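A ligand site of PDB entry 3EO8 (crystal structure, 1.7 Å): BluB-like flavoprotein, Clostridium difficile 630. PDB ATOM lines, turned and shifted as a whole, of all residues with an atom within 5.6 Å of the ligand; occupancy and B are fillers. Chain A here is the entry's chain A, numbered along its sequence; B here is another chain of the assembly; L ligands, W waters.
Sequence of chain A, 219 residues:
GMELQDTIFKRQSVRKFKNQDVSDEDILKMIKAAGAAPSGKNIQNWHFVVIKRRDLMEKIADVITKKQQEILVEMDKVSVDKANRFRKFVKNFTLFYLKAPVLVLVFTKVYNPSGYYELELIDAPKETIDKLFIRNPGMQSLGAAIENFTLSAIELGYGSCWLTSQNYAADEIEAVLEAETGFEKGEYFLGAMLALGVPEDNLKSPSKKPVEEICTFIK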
ATOM      1  N   ARG A  11     -20.293  31.765   8.787  1.00  0.00           N
ATOM      2  CA  ARG A  11     -19.030  31.630   9.476  1.00  0.00           C
ATOM      3  C   ARG A  11     -19.116  30.657  10.647  1.00  0.00           C
ATOM      4  O   ARG A  11     -19.946  30.806  11.567  1.00  0.00           O
ATOM      5  CB  ARG A  11     -18.504  32.974   9.998  1.00  0.00           C
ATOM      6  CG  ARG A  11     -17.085  32.960  10.503  1.00  0.00           C
ATOM      7  CD  ARG A  11     -16.874  33.854  11.695  1.00  0.00           C
ATOM      8  NE  ARG A  11     -17.794  33.541  12.761  1.00  0.00           N
ATOM      9  CZ  ARG A  11     -17.702  32.479  13.546  1.00  0.00           C
ATOM     10  NH1 ARG A  11     -16.686  31.638  13.407  1.00  0.00           N
ATOM     11  NH2 ARG A  11     -18.603  32.289  14.485  1.00  0.00           N
ATOM     12  N   GLN A  12     -18.206  29.691  10.610  1.00  0.00           N
ATOM     13  CA  GLN A  12     -18.001  28.787  11.712  1.00  0.00           C
ATOM     14  C   GLN A  12     -16.499  28.617  11.948  1.00  0.00           C
ATOM     15  O   GLN A  12     -15.685  28.935  11.078  1.00  0.00           O
ATOM     16  CB  GLN A  12     -18.616  27.422  11.345  1.00  0.00           C
ATOM     17  CG  GLN A  12     -20.125  27.410  11.218  1.00  0.00           C
ATOM     18  CD  GLN A  12     -20.645  26.008  10.918  1.00  0.00           C
ATOM     19  OE1 GLN A  12     -20.767  25.633   9.738  1.00  0.00           O
ATOM     20  NE2 GLN A  12     -20.880  25.200  11.959  1.00  0.00           N
ATOM     21  N   SER A  13     -16.109  28.076  13.104  1.00  0.00           N
ATOM     22  CA  SER A  13     -14.717  27.625  13.269  1.00  0.00           C
ATOM     23  C   SER A  13     -14.491  26.280  12.595  1.00  0.00           C
ATOM     24  O   SER A  13     -14.971  25.223  13.059  1.00  0.00           O
ATOM     25  CB  SER A  13     -14.347  27.525  14.747  1.00  0.00           C
ATOM     26  OG  SER A  13     -14.375  28.804  15.283  1.00  0.00           O
ATOM     27  N   ARG A  15     -12.489  23.191  11.491  1.00  0.00           N
ATOM     28  CA  ARG A  15     -11.383  22.379  12.018  1.00  0.00           C
ATOM     29  C   ARG A  15     -11.143  21.112  11.200  1.00  0.00           C
ATOM     30  O   ARG A  15     -10.248  20.330  11.497  1.00  0.00           O
ATOM     31  CB  ARG A  15     -11.604  22.059  13.498  1.00  0.00           C
ATOM     32  CG  ARG A  15     -11.824  23.282  14.348  1.00  0.00           C
ATOM     33  CD  ARG A  15     -11.770  23.005  15.841  1.00  0.00           C
ATOM     34  NE  ARG A  15     -12.006  24.251  16.600  1.00  0.00           N
ATOM     35  CZ  ARG A  15     -13.204  24.757  16.883  1.00  0.00           C
ATOM     36  NH1 ARG A  15     -14.327  24.170  16.490  1.00  0.00           N
ATOM     37  NH2 ARG A  15     -13.280  25.881  17.559  1.00  0.00           N
ATOM     38  N   PHE A  89      -7.353  18.821  24.920  1.00  0.00           N
ATOM     39  CA  PHE A  89      -7.574  20.183  24.410  1.00  0.00           C
ATOM     40  C   PHE A  89      -6.581  20.576  23.296  1.00  0.00           C
ATOM     41  O   PHE A  89      -6.968  21.099  22.241  1.00  0.00           O
ATOM     42  CB  PHE A  89      -7.520  21.197  25.555  1.00  0.00           C
ATOM     43  CG  PHE A  89      -7.542  22.605  25.082  1.00  0.00           C
ATOM     44  CD1 PHE A  89      -8.730  23.230  24.798  1.00  0.00           C
ATOM     45  CD2 PHE A  89      -6.354  23.300  24.866  1.00  0.00           C
ATOM     46  CE1 PHE A  89      -8.744  24.534  24.319  1.00  0.00           C
ATOM     47  CE2 PHE A  89      -6.374  24.591  24.398  1.00  0.00           C
ATOM     48  CZ  PHE A  89      -7.567  25.204  24.125  1.00  0.00           C
ATOM     49  N   ASN A  92      -7.324  18.749  19.989  1.00  0.00           N
ATOM     50  CA  ASN A  92      -8.598  19.085  19.342  1.00  0.00           C
ATOM     51  C   ASN A  92      -8.733  20.547  18.933  1.00  0.00           C
ATOM     52  O   ASN A  92      -9.358  20.859  17.901  1.00  0.00           O
ATOM     53  CB  ASN A  92      -9.723  18.635  20.255  1.00  0.00           C
ATOM     54  CG  ASN A  92      -9.851  17.115  20.290  1.00  0.00           C
ATOM     55  OD1 ASN A  92      -9.445  16.425  19.357  1.00  0.00           O
ATOM     56  ND2 ASN A  92     -10.417  16.587  21.367  1.00  0.00           N
ATOM     57  N   PHE A  93      -8.121  21.416  19.723  1.00  0.00           N
ATOM     58  CA  PHE A  93      -8.227  22.874  19.553  1.00  0.00           C
ATOM     59  C   PHE A  93      -6.908  23.596  19.219  1.00  0.00           C
ATOM     60  O   PHE A  93      -6.868  24.833  19.131  1.00  0.00           O
ATOM     61  CB  PHE A  93      -8.897  23.501  20.795  1.00  0.00           C
ATOM     62  CG  PHE A  93     -10.298  22.991  20.984  1.00  0.00           C
ATOM     63  CD1 PHE A  93     -11.328  23.472  20.187  1.00  0.00           C
ATOM     64  CD2 PHE A  93     -10.577  21.970  21.907  1.00  0.00           C
ATOM     65  CE1 PHE A  93     -12.627  22.969  20.330  1.00  0.00           C
ATOM     66  CE2 PHE A  93     -11.867  21.470  22.060  1.00  0.00           C
ATOM     67  CZ  PHE A  93     -12.890  21.965  21.262  1.00  0.00           C
ATOM     68  N   THR A  94      -5.836  22.871  18.992  1.00  0.00           N
ATOM     69  CA  THR A  94      -4.628  23.545  18.505  1.00  0.00           C
ATOM     70  C   THR A  94      -3.999  22.786  17.312  1.00  0.00           C
ATOM     71  O   THR A  94      -3.910  23.320  16.200  1.00  0.00           O
ATOM     72  CB  THR A  94      -3.554  23.754  19.610  1.00  0.00           C
ATOM     73  OG1 THR A  94      -4.164  24.221  20.835  1.00  0.00           O
ATOM     74  CG2 THR A  94      -2.514  24.782  19.137  1.00  0.00           C
ATOM     75  N   PHE A  96      -4.917  20.598  15.314  1.00  0.00           N
ATOM     76  CA  PHE A  96      -5.764  20.294  14.151  1.00  0.00           C
ATOM     77  C   PHE A  96      -5.440  21.144  12.932  1.00  0.00           C
ATOM     78  O   PHE A  96      -5.834  20.792  11.827  1.00  0.00           O
ATOM     79  CB  PHE A  96      -7.255  20.483  14.474  1.00  0.00           C
ATOM     80  CG  PHE A  96      -7.638  21.902  14.562  1.00  0.00           C
ATOM     81  CD1 PHE A  96      -7.981  22.601  13.417  1.00  0.00           C
ATOM     82  CD2 PHE A  96      -7.578  22.577  15.762  1.00  0.00           C
ATOM     83  CE1 PHE A  96      -8.296  23.917  13.455  1.00  0.00           C
ATOM     84  CE2 PHE A  96      -7.895  23.904  15.820  1.00  0.00           C
ATOM     85  CZ  PHE A  96      -8.235  24.592  14.665  1.00  0.00           C
ATOM     86  N   CYS A 161     -10.260  28.610  10.897  1.00  0.00           N
ATOM     87  CA  CYS A 161     -10.405  28.694  12.324  1.00  0.00           C
ATOM     88  C   CYS A 161      -9.328  29.629  12.765  1.00  0.00           C
ATOM     89  O   CYS A 161      -8.208  29.562  12.286  1.00  0.00           O
ATOM     90  CB  CYS A 161     -10.231  27.350  13.017  1.00  0.00           C
ATOM     91  SG  CYS A 161     -10.628  27.292  14.815  1.00  0.00           S
ATOM     92  N   TRP A 162      -9.723  30.485  13.691  1.00  0.00           N
ATOM     93  CA  TRP A 162      -8.852  31.442  14.372  1.00  0.00           C
ATOM     94  C   TRP A 162      -8.253  30.759  15.583  1.00  0.00           C
ATOM     95  O   TRP A 162      -8.966  30.068  16.295  1.00  0.00           O
ATOM     96  CB  TRP A 162      -9.801  32.553  14.806  1.00  0.00           C
ATOM     97  CG  TRP A 162      -9.277  33.884  15.239  1.00  0.00           C
ATOM     98  CD1 TRP A 162      -8.144  34.171  15.946  1.00  0.00           C
ATOM     99  CD2 TRP A 162      -9.987  35.107  15.113  1.00  0.00           C
ATOM    100  NE1 TRP A 162      -8.081  35.522  16.193  1.00  0.00           N
ATOM    101  CE2 TRP A 162      -9.215  36.109  15.697  1.00  0.00           C
ATOM    102  CE3 TRP A 162     -11.198  35.458  14.511  1.00  0.00           C
ATOM    103  CZ2 TRP A 162      -9.615  37.446  15.720  1.00  0.00           C
ATOM    104  CZ3 TRP A 162     -11.595  36.785  14.514  1.00  0.00           C
ATOM    105  CH2 TRP A 162     -10.802  37.763  15.129  1.00  0.00           C
ATOM    106  N   LEU A 163      -6.947  30.898  15.807  1.00  0.00           N
ATOM    107  CA  LEU A 163      -6.296  30.266  16.952  1.00  0.00           C
ATOM    108  C   LEU A 163      -5.472  31.229  17.767  1.00  0.00           C
ATOM    109  O   LEU A 163      -4.630  31.953  17.237  1.00  0.00           O
ATOM    110  CB  LEU A 163      -5.385  29.140  16.512  1.00  0.00           C
ATOM    111  CG  LEU A 163      -6.043  27.933  15.800  1.00  0.00           C
ATOM    112  CD1 LEU A 163      -6.219  28.108  14.288  1.00  0.00           C
ATOM    113  CD2 LEU A 163      -5.231  26.646  16.104  1.00  0.00           C
ATOM    114  N   THR A 164      -5.657  31.199  19.071  1.00  0.00           N
ATOM    115  CA  THR A 164      -4.710  31.836  19.983  1.00  0.00           C
ATOM    116  C   THR A 164      -4.216  30.840  21.024  1.00  0.00           C
ATOM    117  O   THR A 164      -3.377  31.187  21.865  1.00  0.00           O
ATOM    118  CB  THR A 164      -5.291  33.096  20.651  1.00  0.00           C
ATOM    119  OG1 THR A 164      -6.513  32.797  21.332  1.00  0.00           O
ATOM    120  CG2 THR A 164      -5.490  34.219  19.619  1.00  0.00           C
ATOM    121  N   SER A 165      -4.694  29.601  20.995  1.00  0.00           N
ATOM    122  CA  SER A 165      -4.381  28.631  22.054  1.00  0.00           C
ATOM    123  C   SER A 165      -2.906  28.207  22.022  1.00  0.00           C
ATOM    124  O   SER A 165      -2.410  27.661  22.982  1.00  0.00           O
ATOM    125  CB  SER A 165      -5.278  27.389  22.008  1.00  0.00           C
ATOM    126  OG  SER A 165      -5.156  26.710  20.778  1.00  0.00           O
ATOM    127  N   GLN A 166      -2.220  28.449  20.921  1.00  0.00           N
ATOM    128  CA  GLN A 166      -0.791  28.135  20.847  1.00  0.00           C
ATOM    129  C   GLN A 166       0.120  29.109  21.586  1.00  0.00           C
ATOM    130  O   GLN A 166       1.325  28.873  21.661  1.00  0.00           O
ATOM    131  CB  GLN A 166      -0.360  28.108  19.372  1.00  0.00           C
ATOM    132  CG  GLN A 166      -0.258  29.463  18.684  1.00  0.00           C
ATOM    133  CD  GLN A 166      -1.613  30.097  18.369  1.00  0.00           C
ATOM    134  OE1 GLN A 166      -2.623  29.410  18.254  1.00  0.00           O
ATOM    135  NE2 GLN A 166      -1.619  31.433  18.179  1.00  0.00           N
ATOM    136  N   LYS A 204     -19.964  21.747  12.926  1.00  0.00           N
ATOM    137  CA  LYS A 204     -20.776  22.059  14.089  1.00  0.00           C
ATOM    138  C   LYS A 204     -20.191  23.219  14.877  1.00  0.00           C
ATOM    139  O   LYS A 204     -18.974  23.353  15.025  1.00  0.00           O
ATOM    140  CB  LYS A 204     -20.877  20.828  15.001  1.00  0.00           C
ATOM    141  CG  LYS A 204     -21.458  19.598  14.336  1.00  0.00           C
ATOM    142  CD  LYS A 204     -22.781  19.881  13.614  1.00  0.00           C
ATOM    143  CE  LYS A 204     -23.289  18.646  12.885  1.00  0.00           C
ATOM    144  NZ  LYS A 204     -24.219  19.008  11.766  1.00  0.00           N
ATOM    145  N   SER A 205     -21.080  24.075  15.359  1.00  0.00           N
ATOM    146  CA  SER A 205     -20.732  25.197  16.242  1.00  0.00           C
ATOM    147  C   SER A 205     -21.583  25.099  17.486  1.00  0.00           C
ATOM    148  O   SER A 205     -22.686  24.582  17.448  1.00  0.00           O
ATOM    149  CB  SER A 205     -21.034  26.513  15.558  1.00  0.00           C
ATOM    150  OG  SER A 205     -20.208  26.669  14.433  1.00  0.00           O
ATOM    151  N   PRO A 206     -21.057  25.588  18.618  1.00  0.00           N
ATOM    152  CA  PRO A 206     -21.809  25.538  19.854  1.00  0.00           C
ATOM    153  C   PRO A 206     -23.000  26.481  19.897  1.00  0.00           C
ATOM    154  O   PRO A 206     -23.089  27.415  19.078  1.00  0.00           O
ATOM    155  CB  PRO A 206     -20.777  25.955  20.902  1.00  0.00           C
ATOM    156  CG  PRO A 206     -19.792  26.773  20.180  1.00  0.00           C
ATOM    157  CD  PRO A 206     -19.736  26.204  18.789  1.00  0.00           C
ATOM    158  N   LYS A 208     -25.299  29.488  21.071  1.00  0.00           N
ATOM    159  CA  LYS A 208     -24.976  30.866  21.343  1.00  0.00           C
ATOM    160  C   LYS A 208     -25.999  31.487  22.283  1.00  0.00           C
ATOM    161  O   LYS A 208     -27.141  31.044  22.395  1.00  0.00           O
ATOM    162  CB  LYS A 208     -24.926  31.627  20.023  1.00  0.00           C
ATOM    163  CG  LYS A 208     -23.855  31.119  19.004  1.00  0.00           C
ATOM    164  CD  LYS A 208     -22.480  30.983  19.607  1.00  0.00           C
ATOM    165  CE  LYS A 208     -21.485  30.317  18.630  1.00  0.00           C
ATOM    166  NZ  LYS A 208     -21.223  31.131  17.397  1.00  0.00           N
ATOM    167  N   ALA B  36     -22.862  36.718  16.414  1.00  0.00           N
ATOM    168  CA  ALA B  36     -22.442  35.575  15.631  1.00  0.00           C
ATOM    169  C   ALA B  36     -20.913  35.554  15.398  1.00  0.00           C
ATOM    170  O   ALA B  36     -20.409  34.662  14.748  1.00  0.00           O
ATOM    171  CB  ALA B  36     -23.156  35.620  14.314  1.00  0.00           C
ATOM    172  N   ALA B  37     -20.196  36.544  15.916  1.00  0.00           N
ATOM    173  CA  ALA B  37     -18.750  36.622  15.803  1.00  0.00           C
ATOM    174  C   ALA B  37     -18.088  35.469  16.541  1.00  0.00           C
ATOM    175  O   ALA B  37     -18.640  34.933  17.487  1.00  0.00           O
ATOM    176  CB  ALA B  37     -18.273  37.959  16.359  1.00  0.00           C
ATOM    177  N   PRO B  38     -16.865  35.088  16.100  1.00  0.00           N
ATOM    178  CA  PRO B  38     -16.182  34.039  16.791  1.00  0.00           C
ATOM    179  C   PRO B  38     -15.664  34.637  18.100  1.00  0.00           C
ATOM    180  O   PRO B  38     -15.543  35.868  18.209  1.00  0.00           O
ATOM    181  CB  PRO B  38     -15.030  33.694  15.842  1.00  0.00           C
ATOM    182  CG  PRO B  38     -14.741  34.982  15.147  1.00  0.00           C
ATOM    183  CD  PRO B  38     -16.064  35.643  14.979  1.00  0.00           C
ATOM    184  N   SER B  39     -15.437  33.794  19.097  1.00  0.00           N
ATOM    185  CA  SER B  39     -14.882  34.233  20.361  1.00  0.00           C
ATOM    186  C   SER B  39     -14.151  33.117  21.063  1.00  0.00           C
ATOM    187  O   SER B  39     -14.534  31.977  20.934  1.00  0.00           O
ATOM    188  CB  SER B  39     -15.968  34.818  21.276  1.00  0.00           C
ATOM    189  OG  SER B  39     -16.863  33.869  21.798  1.00  0.00           O
ATOM    190  N   GLY B  40     -13.113  33.465  21.823  1.00  0.00           N
ATOM    191  CA  GLY B  40     -12.292  32.481  22.543  1.00  0.00           C
ATOM    192  C   GLY B  40     -13.144  31.601  23.441  1.00  0.00           C
ATOM    193  O   GLY B  40     -13.885  32.115  24.281  1.00  0.00           O
ATOM    194  N   LYS B  41     -13.052  30.301  23.224  1.00  0.00           N
ATOM    195  CA  LYS B  41     -13.876  29.287  23.936  1.00  0.00           C
ATOM    196  C   LYS B  41     -15.368  29.651  23.991  1.00  0.00           C
ATOM    197  O   LYS B  41     -16.043  29.325  24.954  1.00  0.00           O
ATOM    198  CB  LYS B  41     -13.320  29.000  25.322  1.00  0.00           C
ATOM    199  CG  LYS B  41     -11.956  28.328  25.277  1.00  0.00           C
ATOM    200  CD  LYS B  41     -11.372  28.105  26.649  1.00  0.00           C
ATOM    201  CE  LYS B  41      -9.989  27.461  26.552  1.00  0.00           C
ATOM    202  NZ  LYS B  41      -9.442  27.040  27.854  1.00  0.00           N
ATOM    203  N   ASN B  42     -15.865  30.324  22.955  1.00  0.00           N
ATOM    204  CA  ASN B  42     -17.275  30.728  22.884  1.00  0.00           C
ATOM    205  C   ASN B  42     -17.705  31.587  24.082  1.00  0.00           C
ATOM    206  O   ASN B  42     -18.853  31.558  24.547  1.00  0.00           O
ATOM    207  CB  ASN B  42     -18.184  29.501  22.747  1.00  0.00           C
ATOM    208  CG  ASN B  42     -19.553  29.856  22.215  1.00  0.00           C
ATOM    209  OD1 ASN B  42     -19.730  30.832  21.449  1.00  0.00           O
ATOM    210  ND2 ASN B  42     -20.551  29.068  22.625  1.00  0.00           N
ATOM    211  N   SER B 114      -6.275  30.279  26.745  1.00  0.00           N
ATOM    212  CA  SER B 114      -5.602  28.988  26.886  1.00  0.00           C
ATOM    213  C   SER B 114      -4.188  29.154  27.413  1.00  0.00           C
ATOM    214  O   SER B 114      -3.457  30.041  26.963  1.00  0.00           O
ATOM    215  CB  SER B 114      -5.570  28.271  25.543  1.00  0.00           C
ATOM    216  OG  SER B 114      -6.832  28.387  24.925  1.00  0.00           O
ATOM    217  N   PRO B 137      -6.538  37.736  23.599  1.00  0.00           N
ATOM    218  CA  PRO B 137      -7.569  37.056  22.773  1.00  0.00           C
ATOM    219  C   PRO B 137      -8.990  37.508  23.101  1.00  0.00           C
ATOM    220  O   PRO B 137      -9.836  37.501  22.215  1.00  0.00           O
ATOM    221  CB  PRO B 137      -7.349  35.583  23.108  1.00  0.00           C
ATOM    222  CG  PRO B 137      -5.893  35.493  23.443  1.00  0.00           C
ATOM    223  CD  PRO B 137      -5.660  36.762  24.256  1.00  0.00           C
ATOM    224  N   GLN B 140      -9.403  40.529  20.964  1.00  0.00           N
ATOM    225  CA  GLN B 140      -9.587  40.081  19.570  1.00  0.00           C
ATOM    226  C   GLN B 140     -11.010  39.681  19.315  1.00  0.00           C
ATOM    227  O   GLN B 140     -11.619  40.063  18.278  1.00  0.00           O
ATOM    228  CB  GLN B 140      -8.642  38.917  19.250  1.00  0.00           C
ATOM    229  CG  GLN B 140      -7.164  39.290  19.253  1.00  0.00           C
ATOM    230  CD  GLN B 140      -6.289  38.180  18.693  1.00  0.00           C
ATOM    231  OE1 GLN B 140      -6.585  37.643  17.651  1.00  0.00           O
ATOM    232  NE2 GLN B 140      -5.182  37.866  19.379  1.00  0.00           N
ATOM    233  N   SER B 141     -11.579  38.912  20.252  1.00  0.00           N
ATOM    234  CA  SER B 141     -12.949  38.461  20.147  1.00  0.00           C
ATOM    235  C   SER B 141     -13.890  39.660  20.114  1.00  0.00           C
ATOM    236  O   SER B 141     -14.757  39.742  19.266  1.00  0.00           O
ATOM    237  CB  SER B 141     -13.326  37.547  21.321  1.00  0.00           C
ATOM    238  OG  SER B 141     -12.365  36.520  21.515  1.00  0.00           O
ATOM    239  N   ALA B 144     -13.823  41.293  16.709  1.00  0.00           N
ATOM    240  CA  ALA B 144     -14.563  40.518  15.682  1.00  0.00           C
ATOM    241  C   ALA B 144     -16.059  40.892  15.747  1.00  0.00           C
ATOM    242  O   ALA B 144     -16.715  41.062  14.712  1.00  0.00           O
ATOM    243  CB  ALA B 144     -14.357  38.971  15.880  1.00  0.00           C
HETATM  244  N1  LIG L   1     -10.754  27.666  18.224  1.00  0.00           N
HETATM  245  C1  LIG L   1      -9.858  26.634  18.381  1.00  0.00           C
HETATM  246  O1  LIG L   1     -10.135  25.467  18.088  1.00  0.00           O
HETATM  247  N2  LIG L   1      -8.603  26.898  18.863  1.00  0.00           N
HETATM  248  C2  LIG L   1      -8.214  28.154  19.246  1.00  0.00           C
HETATM  249  O2  LIG L   1      -7.048  28.329  19.656  1.00  0.00           O
HETATM  250  C3  LIG L   1      -9.114  29.196  19.089  1.00  0.00           C
HETATM  251  N3  LIG L   1      -8.742  30.486  19.422  1.00  0.00           N
HETATM  252  C4  LIG L   1      -9.615  31.537  19.232  1.00  0.00           C
HETATM  253  C5  LIG L   1      -9.192  32.805  19.553  1.00  0.00           C
HETATM  254  C6  LIG L   1     -10.041  33.876  19.361  1.00  0.00           C
HETATM  255  C7  LIG L   1      -9.424  35.243  19.336  1.00  0.00           C
HETATM  256  C8  LIG L   1     -11.321  33.664  18.819  1.00  0.00           C
HETATM  257  C9  LIG L   1     -12.082  34.825  18.237  1.00  0.00           C
HETATM  258  C10 LIG L   1     -11.728  32.381  18.487  1.00  0.00           C
HETATM  259  C11 LIG L   1     -10.884  31.298  18.690  1.00  0.00           C
HETATM  260  N4  LIG L   1     -11.268  29.992  18.399  1.00  0.00           N
HETATM  261  C12 LIG L   1     -10.369  28.951  18.546  1.00  0.00           C
HETATM  262  C13 LIG L   1     -12.651  29.667  17.907  1.00  0.00           C
HETATM  263  C14 LIG L   1     -13.696  29.629  19.018  1.00  0.00           C
HETATM  264  O3  LIG L   1     -13.572  28.428  19.777  1.00  0.00           O
HETATM  265  C15 LIG L   1     -15.085  29.684  18.380  1.00  0.00           C
HETATM  266  O4  LIG L   1     -15.216  30.916  17.690  1.00  0.00           O
HETATM  267  C16 LIG L   1     -16.255  29.497  19.344  1.00  0.00           C
HETATM  268  O5  LIG L   1     -16.218  28.216  19.961  1.00  0.00           O
HETATM  269  C17 LIG L   1     -17.563  29.645  18.557  1.00  0.00           C
HETATM  270  O6  LIG L   1     -17.626  28.630  17.573  1.00  0.00           O
HETATM  271  P1  LIG L   1     -17.943  29.051  16.038  1.00  0.00           P
HETATM  272  O7  LIG L   1     -17.985  27.812  15.193  1.00  0.00           O
HETATM  273  O8  LIG L   1     -16.792  29.941  15.624  1.00  0.00           O
HETATM  274  O9  LIG L   1     -19.237  29.842  15.923  1.00  0.00           O
HETATM  275  O   HOH W   1     -20.987  29.768  13.916  1.00  0.00           O
HETATM  276  O   HOH W   2     -16.161  25.876  18.579  1.00  0.00           O
HETATM  277  O   HOH W   3     -18.466  32.717  19.902  1.00  0.00           O
HETATM  278  O   HOH W   4     -17.211  25.442  16.149  1.00  0.00           O
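The side-chain hydroxyl (OG) of Ser 205 is in hydrogen-bond range of an oxygen (O7) of the ligand, 2.6 Å away.
NE of Arg 15 sits at hydrogen-bond distance from O1 of the ligand (2.7 Å).
O7 of the ligand sits at hydrogen-bond distance from N of Ser 13.
The side-chain hydroxyl (OG) of Ser 13 sits at hydrogen-bond distance from an oxygen (O8) of the ligand.
The backbone carbonyl oxygen of Phe 93 lies within hydrogen-bond range of a nitrogen (N2) of the ligand, 2.7 Å away.
N of Ser 165 is in hydrogen-bond range of O2 of the ligand (3.0 Å).
The side-chain hydroxyl of Ser 165 lies within hydrogen-bond range of an oxygen (O2) of the ligand.
NZ of Lys 208 is in salt-bridge range of O9 of the ligand (2.8 Å).
The guanidinium group (NH1) of Arg 11 is in salt-bridge range of an oxygen (O8) of the ligand, at 2.8 Å.
An oxygen (O4) of the ligand lies within hydrogen-bond range of the backbone NH (N) of Ser 39 of chain B.
The backbone carbonyl oxygen (O) of Ser 39 of chain B lies close to an oxygen (O4) of the ligand, 3.5 Å away.
A nitrogen (N3) of the ligand sits at hydrogen-bond distance from the backbone NH of Thr 164, at 3.2 Å.
The side-chain sulfur (SG) of Cys 161 lies within hydrogen-bond range of a nitrogen (N1) of the ligand (3.4 Å).
OG of Ser 205 is in hydrogen-bond range of NE2 of Gln 12 (3.0 Å).
The guanidinium group (NE) of Arg 15 lies within hydrogen-bond range of the side-chain sulfur (SG) of Cys 161 (3.8 Å).
O of Phe 93 is in hydrogen-bond range of OG of Ser 165 (3.0 Å).
The side-chain hydroxyl (OG1) of Thr 94 lies within hydrogen-bond range of the side-chain hydroxyl (OG) of Ser 165 (2.7 Å).
The side-chain amide oxygen (OE1) of Gln 140 of chain B sits at hydrogen-bond distance from the indole nitrogen (NE1) of Trp 162.
O of Leu 163 sits at hydrogen-bond distance from NE2 of Gln 166, at 3.2 Å.
The side-chain hydroxyl (OG) of Ser 141 of chain B is in hydrogen-bond range of the backbone NH (N) of Gly 40 of chain B, at 3.2 Å.
The backbone carbonyl oxygen (O) of Pro 137 of chain B sits at hydrogen-bond distance from the side-chain hydroxyl (OG) of Ser 141 of chain B (2.8 Å).
The backbone carbonyl oxygen (O) of Trp 162 sits close to a nitrogen (N4) of the ligand (3.1 Å).
Merely in contact with the ligand: Pro 38 of chain B (3.3 Å), Leu 163 (3.4 Å), Pro 206 (3.4 Å), Gly 40 of chain B (3.5 Å), Phe 96 (3.6 Å), Gln 12 (3.6 Å), Asn 42 of chain B (3.6 Å), Pro 137 of chain B (3.7 Å), Ser 141 of chain B (3.7 Å), Gln 140 of chain B (3.8 Å) and Lys 41 of chain B (3.96 Å).
Hydrophobic or aromatic side chains within 4 Å of the ligand: Phe 93, Phe 96, Trp 162, Leu 163, Pro 206 and Pro 38 of chain B.
Within 4 Å of the ligand: Arg 11, Gln 12, Ser 13, Arg 15, Phe 93, Phe 96, Cys 161, Trp 162, Leu 163, Thr 164, Ser 165, Ser 205, Pro 206, Lys 208, Pro 38 of chain B, Ser 39 of chain B, Gly 40 of chain B, Lys 41 of chain B, Asn 42 of chain B, Pro 137 of chain B, Gln 140 of chain B and Ser 141 of chain B.
Water W1 lies within hydrogen-bond range of an oxygen (O9) of the ligand, the backbone carbonyl oxygen (O) of Arg 11 and the side-chain hydroxyl (OG) of Ser 205.
Water W4 lies within hydrogen-bond range of O7 of the ligand (2.7 Å), O of Lys 204 (3.0 Å) and NH1 of Arg 15 (3.2 Å).
Water W2 bridges O5 of the ligand (2.7 Å) and NH2 of Arg 15 (3.1 Å).
Water W3 lies within hydrogen-bond range of OG of Ser 39 of chain B (2.7 Å), OD1 of Asn 42 of chain B (2.7 Å) and O of Ala 37 of chain B (3.3 Å).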
